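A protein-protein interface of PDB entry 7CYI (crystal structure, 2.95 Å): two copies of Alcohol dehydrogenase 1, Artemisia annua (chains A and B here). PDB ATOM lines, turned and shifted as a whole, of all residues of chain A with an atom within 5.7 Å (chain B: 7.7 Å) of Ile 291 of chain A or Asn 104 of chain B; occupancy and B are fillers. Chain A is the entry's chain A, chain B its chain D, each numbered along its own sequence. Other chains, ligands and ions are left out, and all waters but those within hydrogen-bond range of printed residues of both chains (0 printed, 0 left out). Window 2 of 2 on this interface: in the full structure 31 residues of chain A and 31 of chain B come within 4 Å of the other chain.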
ATOM      1  N   ASP A 268      14.922  37.223  -5.846  1.00  0.00           N
ATOM      2  CA  ASP A 268      15.678  36.292  -6.676  1.00  0.00           C
ATOM      3  C   ASP A 268      17.030  36.879  -7.057  1.00  0.00           C
ATOM      4  O   ASP A 268      18.069  36.229  -6.901  1.00  0.00           O
ATOM      5  CB  ASP A 268      14.878  35.930  -7.928  1.00  0.00           C
ATOM      6  CG  ASP A 268      13.608  35.163  -7.612  1.00  0.00           C
ATOM      7  OD1 ASP A 268      13.681  34.185  -6.838  1.00  0.00           O
ATOM      8  OD2 ASP A 268      12.538  35.539  -8.137  1.00  0.00           O
ATOM      9  N   LYS A 288      17.634  35.256  -1.861  1.00  0.00           N
ATOM     10  CA  LYS A 288      16.923  34.056  -1.451  1.00  0.00           C
ATOM     11  C   LYS A 288      17.894  32.959  -1.033  1.00  0.00           C
ATOM     12  O   LYS A 288      19.026  32.880  -1.519  1.00  0.00           O
ATOM     13  CB  LYS A 288      16.027  33.546  -2.580  1.00  0.00           C
ATOM     14  CG  LYS A 288      14.669  34.214  -2.663  1.00  0.00           C
ATOM     15  CD  LYS A 288      13.782  33.483  -3.659  1.00  0.00           C
ATOM     16  CE  LYS A 288      12.403  34.110  -3.755  1.00  0.00           C
ATOM     17  NZ  LYS A 288      11.574  33.446  -4.798  1.00  0.00           N
ATOM     18  N   ILE A 289      17.431  32.105  -0.125  1.00  0.00           N
ATOM     19  CA  ILE A 289      18.232  30.985   0.357  1.00  0.00           C
ATOM     20  C   ILE A 289      18.328  29.942  -0.749  1.00  0.00           C
ATOM     21  O   ILE A 289      17.307  29.449  -1.244  1.00  0.00           O
ATOM     22  CB  ILE A 289      17.625  30.377   1.628  1.00  0.00           C
ATOM     23  CG1 ILE A 289      17.573  31.403   2.761  1.00  0.00           C
ATOM     24  CG2 ILE A 289      18.426  29.163   2.061  1.00  0.00           C
ATOM     25  CD1 ILE A 289      18.923  31.957   3.127  1.00  0.00           C
ATOM     26  N   GLY A 290      19.555  29.611  -1.145  1.00  0.00           N
ATOM     27  CA  GLY A 290      19.758  28.511  -2.065  1.00  0.00           C
ATOM     28  C   GLY A 290      19.505  28.814  -3.529  1.00  0.00           C
ATOM     29  O   GLY A 290      20.062  28.146  -4.404  1.00  0.00           O
ATOM     30  N   ILE A 291      18.664  29.810  -3.819  1.00  0.00           N
ATOM     31  CA  ILE A 291      18.353  30.176  -5.195  1.00  0.00           C
ATOM     32  C   ILE A 291      18.569  31.653  -5.480  1.00  0.00           C
ATOM     33  O   ILE A 291      18.363  32.086  -6.615  1.00  0.00           O
ATOM     34  CB  ILE A 291      16.915  29.769  -5.579  1.00  0.00           C
ATOM     35  CG1 ILE A 291      15.893  30.622  -4.833  1.00  0.00           C
ATOM     36  CG2 ILE A 291      16.678  28.295  -5.308  1.00  0.00           C
ATOM     37  CD1 ILE A 291      14.465  30.231  -5.123  1.00  0.00           C
ATOM     38  N   GLY A 292      18.975  32.449  -4.492  1.00  0.00           N
ATOM     39  CA  GLY A 292      19.217  33.858  -4.734  1.00  0.00           C
ATOM     40  C   GLY A 292      20.606  34.114  -5.292  1.00  0.00           C
ATOM     41  O   GLY A 292      21.563  33.398  -5.006  1.00  0.00           O
ATOM     42  N   THR A 293      20.707  35.155  -6.117  1.00  0.00           N
ATOM     43  CA  THR A 293      21.977  35.569  -6.698  1.00  0.00           C
ATOM     44  C   THR A 293      22.216  37.042  -6.402  1.00  0.00           C
ATOM     45  O   THR A 293      21.274  37.840  -6.373  1.00  0.00           O
ATOM     46  CB  THR A 293      22.016  35.329  -8.219  1.00  0.00           C
ATOM     47  OG1 THR A 293      21.386  36.422  -8.894  1.00  0.00           O
ATOM     48  CG2 THR A 293      21.304  34.030  -8.587  1.00  0.00           C
ATOM     49  N   SER A 314      24.682  29.387   2.829  1.00  0.00           N
ATOM     50  CA  SER A 314      23.333  29.701   2.377  1.00  0.00           C
ATOM     51  C   SER A 314      23.058  29.295   0.933  1.00  0.00           C
ATOM     52  O   SER A 314      21.958  29.561   0.437  1.00  0.00           O
ATOM     53  CB  SER A 314      23.064  31.197   2.542  1.00  0.00           C
ATOM     54  OG  SER A 314      24.038  31.973   1.868  1.00  0.00           O
ATOM     55  N   GLY A 315      24.008  28.661   0.249  1.00  0.00           N
ATOM     56  CA  GLY A 315      23.786  28.248  -1.124  1.00  0.00           C
ATOM     57  C   GLY A 315      23.576  29.368  -2.119  1.00  0.00           C
ATOM     58  O   GLY A 315      23.174  29.095  -3.252  1.00  0.00           O
ATOM     59  N   ARG A 316      23.834  30.614  -1.739  1.00  0.00           N
ATOM     60  CA  ARG A 316      23.624  31.742  -2.631  1.00  0.00           C
ATOM     61  C   ARG A 316      24.745  31.833  -3.663  1.00  0.00           C
ATOM     62  O   ARG A 316      25.815  31.237  -3.515  1.00  0.00           O
ATOM     63  CB  ARG A 316      23.543  33.042  -1.835  1.00  0.00           C
ATOM     64  CG  ARG A 316      22.432  33.069  -0.805  1.00  0.00           C
ATOM     65  CD  ARG A 316      22.575  34.276   0.105  1.00  0.00           C
ATOM     66  NE  ARG A 316      21.303  34.668   0.704  1.00  0.00           N
ATOM     67  CZ  ARG A 316      21.029  34.598   2.003  1.00  0.00           C
ATOM     68  NH1 ARG A 316      21.943  34.161   2.855  1.00  0.00           N
ATOM     69  NH2 ARG A 316      19.843  34.985   2.450  1.00  0.00           N
ATOM     70  N   CYS B  99      11.821  17.847   1.936  1.00  0.00           N
ATOM     71  CA  CYS B  99      10.395  17.560   1.825  1.00  0.00           C
ATOM     72  C   CYS B  99       9.981  17.305   0.382  1.00  0.00           C
ATOM     73  O   CYS B  99       9.057  16.524   0.132  1.00  0.00           O
ATOM     74  CB  CYS B  99       9.582  18.712   2.415  1.00  0.00           C
ATOM     75  SG  CYS B  99       9.591  20.215   1.420  1.00  0.00           S
ATOM     76  N   GLY B 100      10.647  17.949  -0.575  1.00  0.00           N
ATOM     77  CA  GLY B 100      10.344  17.773  -1.979  1.00  0.00           C
ATOM     78  C   GLY B 100       9.208  18.615  -2.514  1.00  0.00           C
ATOM     79  O   GLY B 100       8.998  18.636  -3.734  1.00  0.00           O
ATOM     80  N   GLN B 101       8.466  19.318  -1.656  1.00  0.00           N
ATOM     81  CA  GLN B 101       7.301  20.071  -2.092  1.00  0.00           C
ATOM     82  C   GLN B 101       7.362  21.554  -1.754  1.00  0.00           C
ATOM     83  O   GLN B 101       6.397  22.273  -2.041  1.00  0.00           O
ATOM     84  CB  GLN B 101       6.023  19.465  -1.493  1.00  0.00           C
ATOM     85  CG  GLN B 101       6.028  17.943  -1.410  1.00  0.00           C
ATOM     86  CD  GLN B 101       6.024  17.263  -2.777  1.00  0.00           C
ATOM     87  OE1 GLN B 101       5.942  17.919  -3.818  1.00  0.00           O
ATOM     88  NE2 GLN B 101       6.111  15.936  -2.774  1.00  0.00           N
ATOM     89  N   CYS B 102       8.450  22.035  -1.158  1.00  0.00           N
ATOM     90  CA  CYS B 102       8.571  23.455  -0.872  1.00  0.00           C
ATOM     91  C   CYS B 102       9.020  24.210  -2.122  1.00  0.00           C
ATOM     92  O   CYS B 102       9.340  23.621  -3.157  1.00  0.00           O
ATOM     93  CB  CYS B 102       9.544  23.696   0.282  1.00  0.00           C
ATOM     94  SG  CYS B 102      11.278  23.341  -0.091  1.00  0.00           S
ATOM     95  N   LEU B 103       9.039  25.541  -2.015  1.00  0.00           N
ATOM     96  CA  LEU B 103       9.406  26.368  -3.161  1.00  0.00           C
ATOM     97  C   LEU B 103      10.845  26.127  -3.597  1.00  0.00           C
ATOM     98  O   LEU B 103      11.149  26.187  -4.794  1.00  0.00           O
ATOM     99  CB  LEU B 103       9.192  27.846  -2.836  1.00  0.00           C
ATOM    100  CG  LEU B 103       7.778  28.382  -3.055  1.00  0.00           C
ATOM    101  CD1 LEU B 103       7.675  29.825  -2.592  1.00  0.00           C
ATOM    102  CD2 LEU B 103       7.380  28.255  -4.515  1.00  0.00           C
ATOM    103  N   ASN B 104      11.745  25.853  -2.650  1.00  0.00           N
ATOM    104  CA  ASN B 104      13.139  25.615  -3.008  1.00  0.00           C
ATOM    105  C   ASN B 104      13.369  24.203  -3.525  1.00  0.00           C
ATOM    106  O   ASN B 104      14.234  23.999  -4.384  1.00  0.00           O
ATOM    107  CB  ASN B 104      14.046  25.884  -1.807  1.00  0.00           C
ATOM    108  CG  ASN B 104      14.716  27.239  -1.878  1.00  0.00           C
ATOM    109  OD1 ASN B 104      14.238  28.144  -2.561  1.00  0.00           O
ATOM    110  ND2 ASN B 104      15.831  27.384  -1.176  1.00  0.00           N
ATOM    111  N   CYS B 105      12.617  23.221  -3.022  1.00  0.00           N
ATOM    112  CA  CYS B 105      12.801  21.849  -3.484  1.00  0.00           C
ATOM    113  C   CYS B 105      12.270  21.653  -4.897  1.00  0.00           C
ATOM    114  O   CYS B 105      12.778  20.800  -5.633  1.00  0.00           O
ATOM    115  CB  CYS B 105      12.119  20.870  -2.530  1.00  0.00           C
ATOM    116  SG  CYS B 105      13.101  20.409  -1.089  1.00  0.00           S
ATOM    117  N   LYS B 106      11.255  22.424  -5.293  1.00  0.00           N
ATOM    118  CA  LYS B 106      10.653  22.256  -6.610  1.00  0.00           C
ATOM    119  C   LYS B 106      11.480  22.886  -7.722  1.00  0.00           C
ATOM    120  O   LYS B 106      11.261  22.566  -8.896  1.00  0.00           O
ATOM    121  CB  LYS B 106       9.237  22.839  -6.621  1.00  0.00           C
ATOM    122  CG  LYS B 106       8.232  22.028  -5.811  1.00  0.00           C
ATOM    123  CD  LYS B 106       6.811  22.535  -6.010  1.00  0.00           C
ATOM    124  CE  LYS B 106       5.797  21.636  -5.314  1.00  0.00           C
ATOM    125  NZ  LYS B 106       4.394  22.093  -5.532  1.00  0.00           N
ATOM    126  N   THR B 107      12.419  23.771  -7.386  1.00  0.00           N
ATOM    127  CA  THR B 107      13.283  24.348  -8.410  1.00  0.00           C
ATOM    128  C   THR B 107      14.337  23.351  -8.873  1.00  0.00           C
ATOM    129  O   THR B 107      14.708  23.347 -10.051  1.00  0.00           O
ATOM    130  CB  THR B 107      13.953  25.621  -7.890  1.00  0.00           C
ATOM    131  OG1 THR B 107      14.824  25.297  -6.796  1.00  0.00           O
ATOM    132  CG2 THR B 107      12.907  26.620  -7.415  1.00  0.00           C
ATOM    133  N   GLY B 108      14.821  22.501  -7.971  1.00  0.00           N
ATOM    134  CA  GLY B 108      15.844  21.544  -8.337  1.00  0.00           C
ATOM    135  C   GLY B 108      17.227  22.129  -8.479  1.00  0.00           C
ATOM    136  O   GLY B 108      18.109  21.478  -9.050  1.00  0.00           O
ATOM    137  N   LYS B 109      17.446  23.345  -7.978  1.00  0.00           N
ATOM    138  CA  LYS B 109      18.745  23.999  -8.048  1.00  0.00           C
ATOM    139  C   LYS B 109      19.417  24.136  -6.689  1.00  0.00           C
ATOM    140  O   LYS B 109      20.541  24.646  -6.619  1.00  0.00           O
ATOM    141  CB  LYS B 109      18.610  25.384  -8.694  1.00  0.00           C
ATOM    142  CG  LYS B 109      18.287  25.354 -10.181  1.00  0.00           C
ATOM    143  CD  LYS B 109      18.619  26.682 -10.858  1.00  0.00           C
ATOM    144  CE  LYS B 109      17.436  27.644 -10.842  1.00  0.00           C
ATOM    145  NZ  LYS B 109      17.070  28.078  -9.465  1.00  0.00           N
ATOM    146  N   THR B 110      18.765  23.701  -5.613  1.00  0.00           N
ATOM    147  CA  THR B 110      19.336  23.809  -4.280  1.00  0.00           C
ATOM    148  C   THR B 110      18.888  22.619  -3.446  1.00  0.00           C
ATOM    149  O   THR B 110      17.883  21.968  -3.743  1.00  0.00           O
ATOM    150  CB  THR B 110      18.930  25.114  -3.585  1.00  0.00           C
ATOM    151  OG1 THR B 110      19.589  25.203  -2.317  1.00  0.00           O
ATOM    152  CG2 THR B 110      17.426  25.152  -3.364  1.00  0.00           C
ATOM    153  N   ASN B 111      19.653  22.345  -2.391  1.00  0.00           N
ATOM    154  CA  ASN B 111      19.325  21.297  -1.437  1.00  0.00           C
ATOM    155  C   ASN B 111      18.863  21.850  -0.098  1.00  0.00           C
ATOM    156  O   ASN B 111      18.605  21.070   0.825  1.00  0.00           O
ATOM    157  CB  ASN B 111      20.531  20.372  -1.226  1.00  0.00           C
ATOM    158  CG  ASN B 111      21.755  21.110  -0.708  1.00  0.00           C
ATOM    159  OD1 ASN B 111      22.074  22.210  -1.159  1.00  0.00           O
ATOM    160  ND2 ASN B 111      22.446  20.504   0.250  1.00  0.00           N
ATOM    161  N   LEU B 112      18.749  23.172   0.033  1.00  0.00           N
ATOM    162  CA  LEU B 112      18.362  23.807   1.292  1.00  0.00           C
ATOM    163  C   LEU B 112      16.842  23.871   1.347  1.00  0.00           C
ATOM    164  O   LEU B 112      16.220  24.857   0.951  1.00  0.00           O
ATOM    165  CB  LEU B 112      18.992  25.188   1.417  1.00  0.00           C
ATOM    166  CG  LEU B 112      20.503  25.274   1.206  1.00  0.00           C
ATOM    167  CD1 LEU B 112      21.019  26.636   1.614  1.00  0.00           C
ATOM    168  CD2 LEU B 112      21.223  24.189   1.981  1.00  0.00           C
ATOM    169  N   CYS B 113      16.238  22.800   1.855  1.00  0.00           N
ATOM    170  CA  CYS B 113      14.787  22.727   1.957  1.00  0.00           C
ATOM    171  C   CYS B 113      14.265  23.713   2.998  1.00  0.00           C
ATOM    172  O   CYS B 113      14.846  23.872   4.077  1.00  0.00           O
ATOM    173  CB  CYS B 113      14.361  21.304   2.313  1.00  0.00           C
ATOM    174  SG  CYS B 113      12.670  21.163   2.914  1.00  0.00           S
ATOM    175  N   HIS B 114      13.153  24.378   2.662  1.00  0.00           N
ATOM    176  CA  HIS B 114      12.550  25.342   3.577  1.00  0.00           C
ATOM    177  C   HIS B 114      11.898  24.660   4.772  1.00  0.00           C
ATOM    178  O   HIS B 114      11.800  25.259   5.847  1.00  0.00           O
ATOM    179  CB  HIS B 114      11.513  26.191   2.842  1.00  0.00           C
ATOM    180  CG  HIS B 114      12.100  27.169   1.872  1.00  0.00           C
ATOM    181  ND1 HIS B 114      11.400  27.644   0.784  1.00  0.00           N
ATOM    182  CD2 HIS B 114      13.314  27.765   1.828  1.00  0.00           C
ATOM    183  CE1 HIS B 114      12.159  28.490   0.110  1.00  0.00           C
ATOM    184  NE2 HIS B 114      13.326  28.580   0.722  1.00  0.00           N
ATOM    185  N   VAL B 115      11.445  23.416   4.605  1.00  0.00           N
ATOM    186  CA  VAL B 115      10.706  22.743   5.667  1.00  0.00           C
ATOM    187  C   VAL B 115      11.653  22.061   6.646  1.00  0.00           C
ATOM    188  O   VAL B 115      11.395  22.027   7.855  1.00  0.00           O
ATOM    189  CB  VAL B 115       9.704  21.747   5.059  1.00  0.00           C
ATOM    190  CG1 VAL B 115       8.859  21.117   6.149  1.00  0.00           C
ATOM    191  CG2 VAL B 115       8.820  22.448   4.044  1.00  0.00           C
ATOM    192  N   LYS B 319      30.142  30.455  -5.598  1.00  0.00           N
ATOM    193  CA  LYS B 319      28.960  29.648  -5.304  1.00  0.00           C
ATOM    194  C   LYS B 319      29.074  29.136  -3.874  1.00  0.00           C
ATOM    195  O   LYS B 319      29.840  28.213  -3.592  1.00  0.00           O
ATOM    196  CB  LYS B 319      28.832  28.500  -6.302  1.00  0.00           C
ATOM    197  CG  LYS B 319      27.575  27.656  -6.136  1.00  0.00           C
ATOM    198  CD  LYS B 319      26.325  28.444  -6.494  1.00  0.00           C
ATOM    199  CE  LYS B 319      25.074  27.591  -6.359  1.00  0.00           C
ATOM    200  NZ  LYS B 319      24.852  27.141  -4.958  1.00  0.00           N
ATOM    201  N   ARG B 327      21.274  16.718  -2.389  1.00  0.00           N
ATOM    202  CA  ARG B 327      19.926  16.577  -1.855  1.00  0.00           C
ATOM    203  C   ARG B 327      19.834  15.259  -1.094  1.00  0.00           C
ATOM    204  O   ARG B 327      20.105  14.191  -1.655  1.00  0.00           O
ATOM    205  CB  ARG B 327      18.898  16.643  -2.983  1.00  0.00           C
ATOM    206  CG  ARG B 327      18.720  18.042  -3.558  1.00  0.00           C
ATOM    207  CD  ARG B 327      17.755  18.052  -4.726  1.00  0.00           C
ATOM    208  NE  ARG B 327      18.312  17.378  -5.895  1.00  0.00           N
ATOM    209  CZ  ARG B 327      17.667  17.228  -7.048  1.00  0.00           C
ATOM    210  NH1 ARG B 327      16.437  17.705  -7.192  1.00  0.00           N
ATOM    211  NH2 ARG B 327      18.254  16.598  -8.058  1.00  0.00           N
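The backbone carbonyl oxygen (O) of Gly 315 of chain A sits at hydrogen-bond distance from the side-chain amino group (NZ) of Lys 319 of chain B (3.1 Å). ND2 of Asn 104 of chain B sits at hydrogen-bond distance from O of Ile 289 of chain A.
NH1 of Arg 316 of chain A lies close to OG of Ser 314 of chain A. The backbone carbonyl oxygen of Leu 112 of chain B lies within hydrogen-bond range of the side-chain amide nitrogen of Asn 104 of chain B, 3.3 Å away. The side-chain hydroxyl of Thr 107 of chain B is in hydrogen-bond range of the backbone carbonyl oxygen of Asn 104 of chain B (2.8 Å). The backbone carbonyl oxygen (O) of Ser 314 of chain A is in hydrogen-bond range of the backbone NH (N) of Gly 290 of chain A (2.9 Å). The backbone NH (N) of Lys 109 of chain B lies close to the side-chain hydroxyl (OG1) of Thr 107 of chain B. The side-chain amide nitrogen (ND2) of Asn 104 of chain B lies close to a ring nitrogen (NE2) of His 114 of chain B, at 3.4 Å.
CG2 of Ile 289 of chain A touches CD1 of Leu 112 of chain B, 3.6 Å away. Thr 110 of chain B touches Gly 290 of chain A (OG1 to CA, 3.3 Å). CD1 of Ile 291 of chain A touches OD1 of Asn 104 of chain B, 3.3 Å away. OG1 of Thr 107 of chain B touches CG2 of Ile 291 of chain A (3.8 Å). Thr 110 of chain B touches Ile 291 of chain A (CG2 to CG2, 3.8 Å). Ser 314 of chain A touches Leu 112 of chain B (O to CD1, 3.3 Å). Gly 315 of chain A touches Leu 112 of chain B (N to CD1, 3.9 Å). O of Arg 316 of chain A touches C of Lys 319 of chain B, at 3.9 Å.
Gly 290 of chain A touches one residue of chain B. Ile 291 of chain A touches just these residues of chain B: Asn 104, Thr 107 and Thr 110. No residue of chain B comes within 4 Å of Gly 292 of chain A. Thr 293 of chain A touches none of the printed residues of chain B. Printed residues of chain B within 4 Å of Ser 314 of chain A: Leu 112 (3.3 Å). Gln 101 of chain B touches none of the printed residues of chain A. Of chain A, only Ile 289 and Ile 291 come within 4 Å of Asn 104 of chain B. Printed residues of chain A within 4 Å of Thr 107 of chain B: Ile 291 (3.8 Å). Of the printed residues of chain A, Lys 319 of chain B touches Gly 315 and Arg 316. The nearest residue of chain B that does not touch Ile 291 of chain A is Lys 109 of chain B (4.2 Å). The nearest residue of chain A that does not touch Asn 104 of chain B is Gly 290 of chain A (4.2 Å).
Of the 10 printed residues of chain A, 6 touch a printed residue of chain B. Hydrophobic or aromatic side chains of chain A within 4 Å of the printed part of chain B: Ile 289 and Ile 291. Of the 19 printed residues of chain B, 5 touch a printed residue of chain A. Printed residues of chain B that touch a printed residue of chain A: Asn 104, Thr 107, Thr 110, Leu 112 and Lys 319. Hydrophobic or aromatic side chains of chain B within 4 Å of the printed part of chain A: Leu 112. Among the printed residues, 10 pairs touch across the chains.
No position is printed for both chains. Of the 10 pairs that touch across the chains among the printed residues, none has its exchanged pair printed and touching as well.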
